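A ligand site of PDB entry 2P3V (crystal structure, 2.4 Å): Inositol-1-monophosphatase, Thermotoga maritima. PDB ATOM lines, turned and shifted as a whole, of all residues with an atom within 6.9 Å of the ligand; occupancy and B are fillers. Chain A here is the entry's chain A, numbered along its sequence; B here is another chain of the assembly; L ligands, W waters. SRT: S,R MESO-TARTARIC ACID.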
ATOM      1  N   ASP A  36     -21.955  -3.691  23.722  1.00  0.00           N
ATOM      2  CA  ASP A  36     -23.333  -3.327  23.435  1.00  0.00           C
ATOM      3  C   ASP A  36     -23.442  -1.920  22.822  1.00  0.00           C
ATOM      4  O   ASP A  36     -22.440  -1.217  22.666  1.00  0.00           O
ATOM      5  CB  ASP A  36     -24.172  -3.399  24.709  1.00  0.00           C
ATOM      6  CG  ASP A  36     -25.498  -4.121  24.505  1.00  0.00           C
ATOM      7  OD1 ASP A  36     -26.332  -3.659  23.685  1.00  0.00           O
ATOM      8  OD2 ASP A  36     -25.726  -5.157  25.162  1.00  0.00           O
ATOM      9  N   ASP A  82     -34.426  -3.657  26.432  1.00  0.00           N
ATOM     10  CA  ASP A  82     -33.527  -4.749  26.722  1.00  0.00           C
ATOM     11  C   ASP A  82     -33.442  -5.551  25.429  1.00  0.00           C
ATOM     12  O   ASP A  82     -34.441  -6.112  24.977  1.00  0.00           O
ATOM     13  CB  ASP A  82     -34.079  -5.597  27.867  1.00  0.00           C
ATOM     14  CG  ASP A  82     -33.147  -6.721  28.254  1.00  0.00           C
ATOM     15  OD1 ASP A  82     -32.142  -6.922  27.547  1.00  0.00           O
ATOM     16  OD2 ASP A  82     -33.419  -7.397  29.272  1.00  0.00           O
ATOM     17  N   GLY A  83     -32.260  -5.586  24.823  1.00  0.00           N
ATOM     18  CA  GLY A  83     -32.080  -6.282  23.553  1.00  0.00           C
ATOM     19  C   GLY A  83     -31.983  -5.212  22.485  1.00  0.00           C
ATOM     20  O   GLY A  83     -32.489  -5.352  21.373  1.00  0.00           O
ATOM     21  N   THR A  84     -31.316  -4.120  22.848  1.00  0.00           N
ATOM     22  CA  THR A  84     -31.123  -2.983  21.959  1.00  0.00           C
ATOM     23  C   THR A  84     -30.581  -3.444  20.611  1.00  0.00           C
ATOM     24  O   THR A  84     -31.018  -2.971  19.558  1.00  0.00           O
ATOM     25  CB  THR A  84     -30.153  -1.969  22.561  1.00  0.00           C
ATOM     26  OG1 THR A  84     -30.330  -1.931  23.980  1.00  0.00           O
ATOM     27  CG2 THR A  84     -30.414  -0.584  21.983  1.00  0.00           C
ATOM     28  N   ILE A  85     -29.638  -4.375  20.658  1.00  0.00           N
ATOM     29  CA  ILE A  85     -29.059  -4.892  19.435  1.00  0.00           C
ATOM     30  C   ILE A  85     -30.132  -5.542  18.579  1.00  0.00           C
ATOM     31  O   ILE A  85     -30.231  -5.258  17.371  1.00  0.00           O
ATOM     32  CB  ILE A  85     -27.948  -5.904  19.747  1.00  0.00           C
ATOM     33  CG1 ILE A  85     -26.798  -5.165  20.453  1.00  0.00           C
ATOM     34  CG2 ILE A  85     -27.501  -6.616  18.461  1.00  0.00           C
ATOM     35  CD1 ILE A  85     -25.610  -6.060  20.820  1.00  0.00           C
ATOM     36  N   ASN A  86     -30.947  -6.406  19.184  1.00  0.00           N
ATOM     37  CA  ASN A  86     -32.007  -7.051  18.430  1.00  0.00           C
ATOM     38  C   ASN A  86     -32.924  -5.974  17.867  1.00  0.00           C
ATOM     39  O   ASN A  86     -33.239  -5.994  16.671  1.00  0.00           O
ATOM     40  CB  ASN A  86     -32.808  -8.021  19.285  1.00  0.00           C
ATOM     41  CG  ASN A  86     -32.109  -9.352  19.434  1.00  0.00           C
ATOM     42  OD1 ASN A  86     -31.264  -9.701  18.607  1.00  0.00           O
ATOM     43  ND2 ASN A  86     -32.467 -10.108  20.462  1.00  0.00           N
ATOM     44  N   THR A 150     -28.890 -18.844  27.483  1.00  0.00           N
ATOM     45  CA  THR A 150     -27.906 -17.996  28.127  1.00  0.00           C
ATOM     46  C   THR A 150     -27.722 -16.719  27.324  1.00  0.00           C
ATOM     47  O   THR A 150     -28.292 -16.549  26.245  1.00  0.00           O
ATOM     48  CB  THR A 150     -26.543 -18.713  28.235  1.00  0.00           C
ATOM     49  OG1 THR A 150     -25.630 -17.896  28.965  1.00  0.00           O
ATOM     50  CG2 THR A 150     -25.967 -18.991  26.857  1.00  0.00           C
ATOM     51  N   GLY A 151     -26.928 -15.803  27.881  1.00  0.00           N
ATOM     52  CA  GLY A 151     -26.670 -14.562  27.187  1.00  0.00           C
ATOM     53  C   GLY A 151     -25.395 -14.694  26.361  1.00  0.00           C
ATOM     54  O   GLY A 151     -24.724 -15.732  26.411  1.00  0.00           O
ATOM     55  N   SER A 152     -25.073 -13.653  25.605  1.00  0.00           N
ATOM     56  CA  SER A 152     -23.875 -13.657  24.782  1.00  0.00           C
ATOM     57  C   SER A 152     -22.703 -13.060  25.563  1.00  0.00           C
ATOM     58  O   SER A 152     -22.543 -11.834  25.629  1.00  0.00           O
ATOM     59  CB  SER A 152     -24.119 -12.879  23.494  1.00  0.00           C
ATOM     60  OG  SER A 152     -25.028 -13.571  22.667  1.00  0.00           O
ATOM     61  N   TYR A 153     -21.891 -13.931  26.167  1.00  0.00           N
ATOM     62  CA  TYR A 153     -20.733 -13.520  26.958  1.00  0.00           C
ATOM     63  C   TYR A 153     -19.444 -14.141  26.421  1.00  0.00           C
ATOM     64  O   TYR A 153     -19.334 -15.366  26.269  1.00  0.00           O
ATOM     65  CB  TYR A 153     -20.940 -13.930  28.418  1.00  0.00           C
ATOM     66  CG  TYR A 153     -22.347 -13.668  28.914  1.00  0.00           C
ATOM     67  CD1 TYR A 153     -22.904 -12.389  28.852  1.00  0.00           C
ATOM     68  CD2 TYR A 153     -23.144 -14.712  29.399  1.00  0.00           C
ATOM     69  CE1 TYR A 153     -24.214 -12.145  29.247  1.00  0.00           C
ATOM     70  CE2 TYR A 153     -24.467 -14.475  29.793  1.00  0.00           C
ATOM     71  CZ  TYR A 153     -24.992 -13.194  29.721  1.00  0.00           C
ATOM     72  OH  TYR A 153     -26.295 -12.962  30.115  1.00  0.00           O
ATOM     73  N   ILE A 173     -30.077 -18.769  22.438  1.00  0.00           N
ATOM     74  CA  ILE A 173     -29.486 -17.471  22.671  1.00  0.00           C
ATOM     75  C   ILE A 173     -30.461 -16.546  21.939  1.00  0.00           C
ATOM     76  O   ILE A 173     -30.440 -16.453  20.702  1.00  0.00           O
ATOM     77  CB  ILE A 173     -28.059 -17.352  22.097  1.00  0.00           C
ATOM     78  CG1 ILE A 173     -27.141 -18.395  22.735  1.00  0.00           C
ATOM     79  CG2 ILE A 173     -27.507 -15.976  22.388  1.00  0.00           C
ATOM     80  CD1 ILE A 173     -25.745 -18.445  22.152  1.00  0.00           C
ATOM     81  N   LEU A 174     -31.323 -15.903  22.718  1.00  0.00           N
ATOM     82  CA  LEU A 174     -32.387 -15.041  22.209  1.00  0.00           C
ATOM     83  C   LEU A 174     -32.081 -13.563  22.084  1.00  0.00           C
ATOM     84  O   LEU A 174     -32.635 -12.896  21.201  1.00  0.00           O
ATOM     85  CB  LEU A 174     -33.628 -15.217  23.072  1.00  0.00           C
ATOM     86  CG  LEU A 174     -34.060 -16.666  23.278  1.00  0.00           C
ATOM     87  CD1 LEU A 174     -35.203 -16.696  24.260  1.00  0.00           C
ATOM     88  CD2 LEU A 174     -34.472 -17.282  21.945  1.00  0.00           C
ATOM     89  N   GLY A 175     -31.252 -13.033  22.972  1.00  0.00           N
ATOM     90  CA  GLY A 175     -30.897 -11.637  22.880  1.00  0.00           C
ATOM     91  C   GLY A 175     -31.610 -10.570  23.697  1.00  0.00           C
ATOM     92  O   GLY A 175     -31.401  -9.376  23.459  1.00  0.00           O
ATOM     93  N   SER A 176     -32.467 -10.967  24.644  1.00  0.00           N
ATOM     94  CA  SER A 176     -33.149 -10.011  25.521  1.00  0.00           C
ATOM     95  C   SER A 176     -33.168 -10.628  26.922  1.00  0.00           C
ATOM     96  O   SER A 176     -33.946 -11.528  27.192  1.00  0.00           O
ATOM     97  CB  SER A 176     -34.574  -9.725  25.033  1.00  0.00           C
ATOM     98  OG  SER A 176     -35.195  -8.736  25.833  1.00  0.00           O
ATOM     99  N   ALA A 177     -32.312 -10.148  27.815  1.00  0.00           N
ATOM    100  CA  ALA A 177     -32.211 -10.712  29.164  1.00  0.00           C
ATOM    101  C   ALA A 177     -33.478 -10.832  29.973  1.00  0.00           C
ATOM    102  O   ALA A 177     -33.797 -11.917  30.462  1.00  0.00           O
ATOM    103  CB  ALA A 177     -31.168  -9.951  29.961  1.00  0.00           C
ATOM    104  N   ASN A 180     -36.003 -13.400  28.488  1.00  0.00           N
ATOM    105  CA  ASN A 180     -35.487 -14.751  28.652  1.00  0.00           C
ATOM    106  C   ASN A 180     -35.754 -15.222  30.075  1.00  0.00           C
ATOM    107  O   ASN A 180     -36.150 -16.378  30.293  1.00  0.00           O
ATOM    108  CB  ASN A 180     -33.984 -14.738  28.349  1.00  0.00           C
ATOM    109  CG  ASN A 180     -33.506 -16.037  27.693  1.00  0.00           C
ATOM    110  OD1 ASN A 180     -32.512 -16.030  26.948  1.00  0.00           O
ATOM    111  ND2 ASN A 180     -34.167 -17.144  28.003  1.00  0.00           N
ATOM    112  N   PHE A 192     -32.086 -20.346  32.672  1.00  0.00           N
ATOM    113  CA  PHE A 192     -31.462 -19.209  32.013  1.00  0.00           C
ATOM    114  C   PHE A 192     -30.245 -18.741  32.801  1.00  0.00           C
ATOM    115  O   PHE A 192     -30.347 -18.405  33.983  1.00  0.00           O
ATOM    116  CB  PHE A 192     -32.478 -18.066  31.867  1.00  0.00           C
ATOM    117  CG  PHE A 192     -31.873 -16.789  31.334  1.00  0.00           C
ATOM    118  CD1 PHE A 192     -31.208 -16.776  30.110  1.00  0.00           C
ATOM    119  CD2 PHE A 192     -31.967 -15.605  32.065  1.00  0.00           C
ATOM    120  CE1 PHE A 192     -30.642 -15.596  29.606  1.00  0.00           C
ATOM    121  CE2 PHE A 192     -31.402 -14.427  31.580  1.00  0.00           C
ATOM    122  CZ  PHE A 192     -30.749 -14.420  30.346  1.00  0.00           C
ATOM    123  N   VAL A 193     -29.099 -18.716  32.131  1.00  0.00           N
ATOM    124  CA  VAL A 193     -27.832 -18.314  32.721  1.00  0.00           C
ATOM    125  C   VAL A 193     -27.358 -16.985  32.161  1.00  0.00           C
ATOM    126  O   VAL A 193     -27.327 -16.793  30.955  1.00  0.00           O
ATOM    127  CB  VAL A 193     -26.764 -19.372  32.445  1.00  0.00           C
ATOM    128  CG1 VAL A 193     -25.457 -18.941  33.039  1.00  0.00           C
ATOM    129  CG2 VAL A 193     -27.204 -20.693  33.027  1.00  0.00           C
ATOM    130  N   THR A 194     -26.966 -16.069  33.043  1.00  0.00           N
ATOM    131  CA  THR A 194     -26.514 -14.751  32.632  1.00  0.00           C
ATOM    132  C   THR A 194     -25.291 -14.332  33.465  1.00  0.00           C
ATOM    133  O   THR A 194     -25.391 -14.168  34.678  1.00  0.00           O
ATOM    134  CB  THR A 194     -27.656 -13.728  32.763  1.00  0.00           C
ATOM    135  OG1 THR A 194     -27.230 -12.456  32.286  1.00  0.00           O
ATOM    136  CG2 THR A 194     -28.108 -13.632  34.214  1.00  0.00           C
ATOM    137  N   TRP A 195     -24.157 -14.176  32.789  1.00  0.00           N
ATOM    138  CA  TRP A 195     -22.877 -13.837  33.423  1.00  0.00           C
ATOM    139  C   TRP A 195     -22.570 -12.330  33.503  1.00  0.00           C
ATOM    140  O   TRP A 195     -23.205 -11.525  32.824  1.00  0.00           O
ATOM    141  CB  TRP A 195     -21.760 -14.569  32.660  1.00  0.00           C
ATOM    142  CG  TRP A 195     -20.419 -14.654  33.359  1.00  0.00           C
ATOM    143  CD1 TRP A 195     -20.179 -15.063  34.637  1.00  0.00           C
ATOM    144  CD2 TRP A 195     -19.137 -14.426  32.764  1.00  0.00           C
ATOM    145  NE1 TRP A 195     -18.822 -15.111  34.879  1.00  0.00           N
ATOM    146  CE2 TRP A 195     -18.159 -14.729  33.745  1.00  0.00           C
ATOM    147  CE3 TRP A 195     -18.714 -13.998  31.491  1.00  0.00           C
ATOM    148  CZ2 TRP A 195     -16.784 -14.620  33.491  1.00  0.00           C
ATOM    149  CZ3 TRP A 195     -17.348 -13.888  31.246  1.00  0.00           C
ATOM    150  CH2 TRP A 195     -16.395 -14.206  32.246  1.00  0.00           C
ATOM    151  N   ILE A 197     -23.225  -9.383  34.718  1.00  0.00           N
ATOM    152  CA  ILE A 197     -24.198  -8.361  34.319  1.00  0.00           C
ATOM    153  C   ILE A 197     -24.767  -7.599  35.498  1.00  0.00           C
ATOM    154  O   ILE A 197     -24.740  -8.085  36.633  1.00  0.00           O
ATOM    155  CB  ILE A 197     -25.359  -8.991  33.524  1.00  0.00           C
ATOM    156  CG1 ILE A 197     -25.828 -10.276  34.230  1.00  0.00           C
ATOM    157  CG2 ILE A 197     -24.944  -9.245  32.085  1.00  0.00           C
ATOM    158  CD1 ILE A 197     -26.481 -10.045  35.581  1.00  0.00           C
ATOM    159  N   ASP A 201     -30.664  -5.064  36.500  1.00  0.00           N
ATOM    160  CA  ASP A 201     -31.094  -5.389  35.149  1.00  0.00           C
ATOM    161  C   ASP A 201     -32.200  -6.428  35.115  1.00  0.00           C
ATOM    162  O   ASP A 201     -33.048  -6.396  34.228  1.00  0.00           O
ATOM    163  CB  ASP A 201     -29.906  -5.916  34.329  1.00  0.00           C
ATOM    164  CG  ASP A 201     -29.183  -4.827  33.565  1.00  0.00           C
ATOM    165  OD1 ASP A 201     -28.049  -5.094  33.095  1.00  0.00           O
ATOM    166  OD2 ASP A 201     -29.753  -3.724  33.414  1.00  0.00           O
ATOM    167  N   ARG B 169     -20.661  -8.885  16.509  1.00  0.00           N
ATOM    168  CA  ARG B 169     -21.351  -8.101  17.527  1.00  0.00           C
ATOM    169  C   ARG B 169     -22.103  -9.052  18.456  1.00  0.00           C
ATOM    170  O   ARG B 169     -22.019  -8.934  19.678  1.00  0.00           O
ATOM    171  CB  ARG B 169     -22.335  -7.140  16.869  1.00  0.00           C
ATOM    172  CG  ARG B 169     -23.072  -6.228  17.820  1.00  0.00           C
ATOM    173  CD  ARG B 169     -23.929  -5.222  17.069  1.00  0.00           C
ATOM    174  NE  ARG B 169     -23.127  -4.255  16.335  1.00  0.00           N
ATOM    175  CZ  ARG B 169     -23.648  -3.341  15.509  1.00  0.00           C
ATOM    176  NH1 ARG B 169     -24.959  -3.281  15.320  1.00  0.00           N
ATOM    177  NH2 ARG B 169     -22.849  -2.491  14.882  1.00  0.00           N
ATOM    178  N   ARG B 170     -22.842  -9.991  17.867  1.00  0.00           N
ATOM    179  CA  ARG B 170     -23.624 -10.995  18.598  1.00  0.00           C
ATOM    180  C   ARG B 170     -23.912 -12.157  17.671  1.00  0.00           C
ATOM    181  O   ARG B 170     -23.880 -12.027  16.448  1.00  0.00           O
ATOM    182  CB  ARG B 170     -24.966 -10.446  19.075  1.00  0.00           C
ATOM    183  CG  ARG B 170     -24.920  -9.548  20.291  1.00  0.00           C
ATOM    184  CD  ARG B 170     -24.423 -10.282  21.528  1.00  0.00           C
ATOM    185  NE  ARG B 170     -24.601  -9.473  22.730  1.00  0.00           N
ATOM    186  CZ  ARG B 170     -23.937  -8.348  22.996  1.00  0.00           C
ATOM    187  NH1 ARG B 170     -23.039  -7.890  22.137  1.00  0.00           N
ATOM    188  NH2 ARG B 170     -24.198  -7.671  24.101  1.00  0.00           N
ATOM    189  N   ILE B 171     -24.196 -13.308  18.284  1.00  0.00           N
ATOM    190  CA  ILE B 171     -24.535 -14.544  17.579  1.00  0.00           C
ATOM    191  C   ILE B 171     -25.835 -15.044  18.215  1.00  0.00           C
ATOM    192  O   ILE B 171     -25.917 -15.202  19.434  1.00  0.00           O
ATOM    193  CB  ILE B 171     -23.445 -15.618  17.754  1.00  0.00           C
ATOM    194  CG1 ILE B 171     -22.172 -15.202  17.018  1.00  0.00           C
ATOM    195  CG2 ILE B 171     -23.946 -16.951  17.227  1.00  0.00           C
ATOM    196  CD1 ILE B 171     -22.302 -15.148  15.513  1.00  0.00           C
ATOM    197  N   ARG B 172     -26.848 -15.286  17.395  1.00  0.00           N
ATOM    198  CA  ARG B 172     -28.134 -15.765  17.902  1.00  0.00           C
ATOM    199  C   ARG B 172     -28.376 -17.219  17.558  1.00  0.00           C
ATOM    200  O   ARG B 172     -27.862 -17.722  16.567  1.00  0.00           O
ATOM    201  CB  ARG B 172     -29.278 -14.924  17.329  1.00  0.00           C
ATOM    202  CG  ARG B 172     -29.272 -13.459  17.731  1.00  0.00           C
ATOM    203  CD  ARG B 172     -29.544 -13.253  19.217  1.00  0.00           C
ATOM    204  NE  ARG B 172     -29.449 -11.841  19.574  1.00  0.00           N
ATOM    205  CZ  ARG B 172     -28.542 -11.327  20.402  1.00  0.00           C
ATOM    206  NH1 ARG B 172     -28.534 -10.023  20.645  1.00  0.00           N
ATOM    207  NH2 ARG B 172     -27.663 -12.113  21.006  1.00  0.00           N
HETATM  208  O1  SRT L   1     -27.617 -11.400  28.309  1.00  0.00           O
HETATM  209  O11 SRT L   1     -27.388  -9.131  28.813  1.00  0.00           O
HETATM  210  C1  SRT L   1     -27.306 -10.109  28.053  1.00  0.00           C
HETATM  211  C2  SRT L   1     -26.807  -9.978  26.608  1.00  0.00           C
HETATM  212  O2  SRT L   1     -26.492  -8.609  26.492  1.00  0.00           O
HETATM  213  C3  SRT L   1     -27.950 -10.400  25.605  1.00  0.00           C
HETATM  214  O3  SRT L   1     -28.408 -11.795  25.776  1.00  0.00           O
HETATM  215  C4  SRT L   1     -27.390 -10.239  24.194  1.00  0.00           C
HETATM  216  O4  SRT L   1     -27.470  -8.994  23.806  1.00  0.00           O
HETATM  217  O41 SRT L   1     -26.938 -11.141  23.541  1.00  0.00           O
HETATM  218  O   HOH W   1     -28.089  -8.728  31.993  1.00  0.00           O
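The side-chain hydroxyl (OH) of Tyr 153 lies within hydrogen-bond range of an oxygen (O1) of the ligand (2.7 Å). O41 of the ligand is in salt-bridge range of NH2 of Arg 172 of chain B (2.8 Å). The guanidinium group (NE) of Arg 170 of chain B is in salt-bridge range of an oxygen (O41) of the ligand. OG of Ser 152 is in hydrogen-bond range of O41 of the ligand (3.2 Å).
The side-chain hydroxyl (OH) of Tyr 153 lies within hydrogen-bond range of the side-chain hydroxyl (OG1) of Thr 194 (2.4 Å). The guanidinium group (NH2) of Arg 172 of chain B is in hydrogen-bond range of the side-chain hydroxyl (OG) of Ser 152 (3.4 Å). NE of Arg 172 of chain B lies within hydrogen-bond range of OD1 of Asn 86 (3.0 Å). The guanidinium group (NH2) of Arg 170 of chain B is in salt-bridge range of the side-chain carboxylate (OD2) of Asp 36. The backbone carbonyl oxygen (O) of Val 193 lies within hydrogen-bond range of the backbone NH (N) of Gly 151, at 3.3 Å. The side-chain amide nitrogen (ND2) of Asn 86 lies close to the backbone carbonyl oxygen (O) of Gly 175 (3.3 Å).
Residues that only touch the ligand: Gly 151, Asp 36 and Gly 175.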
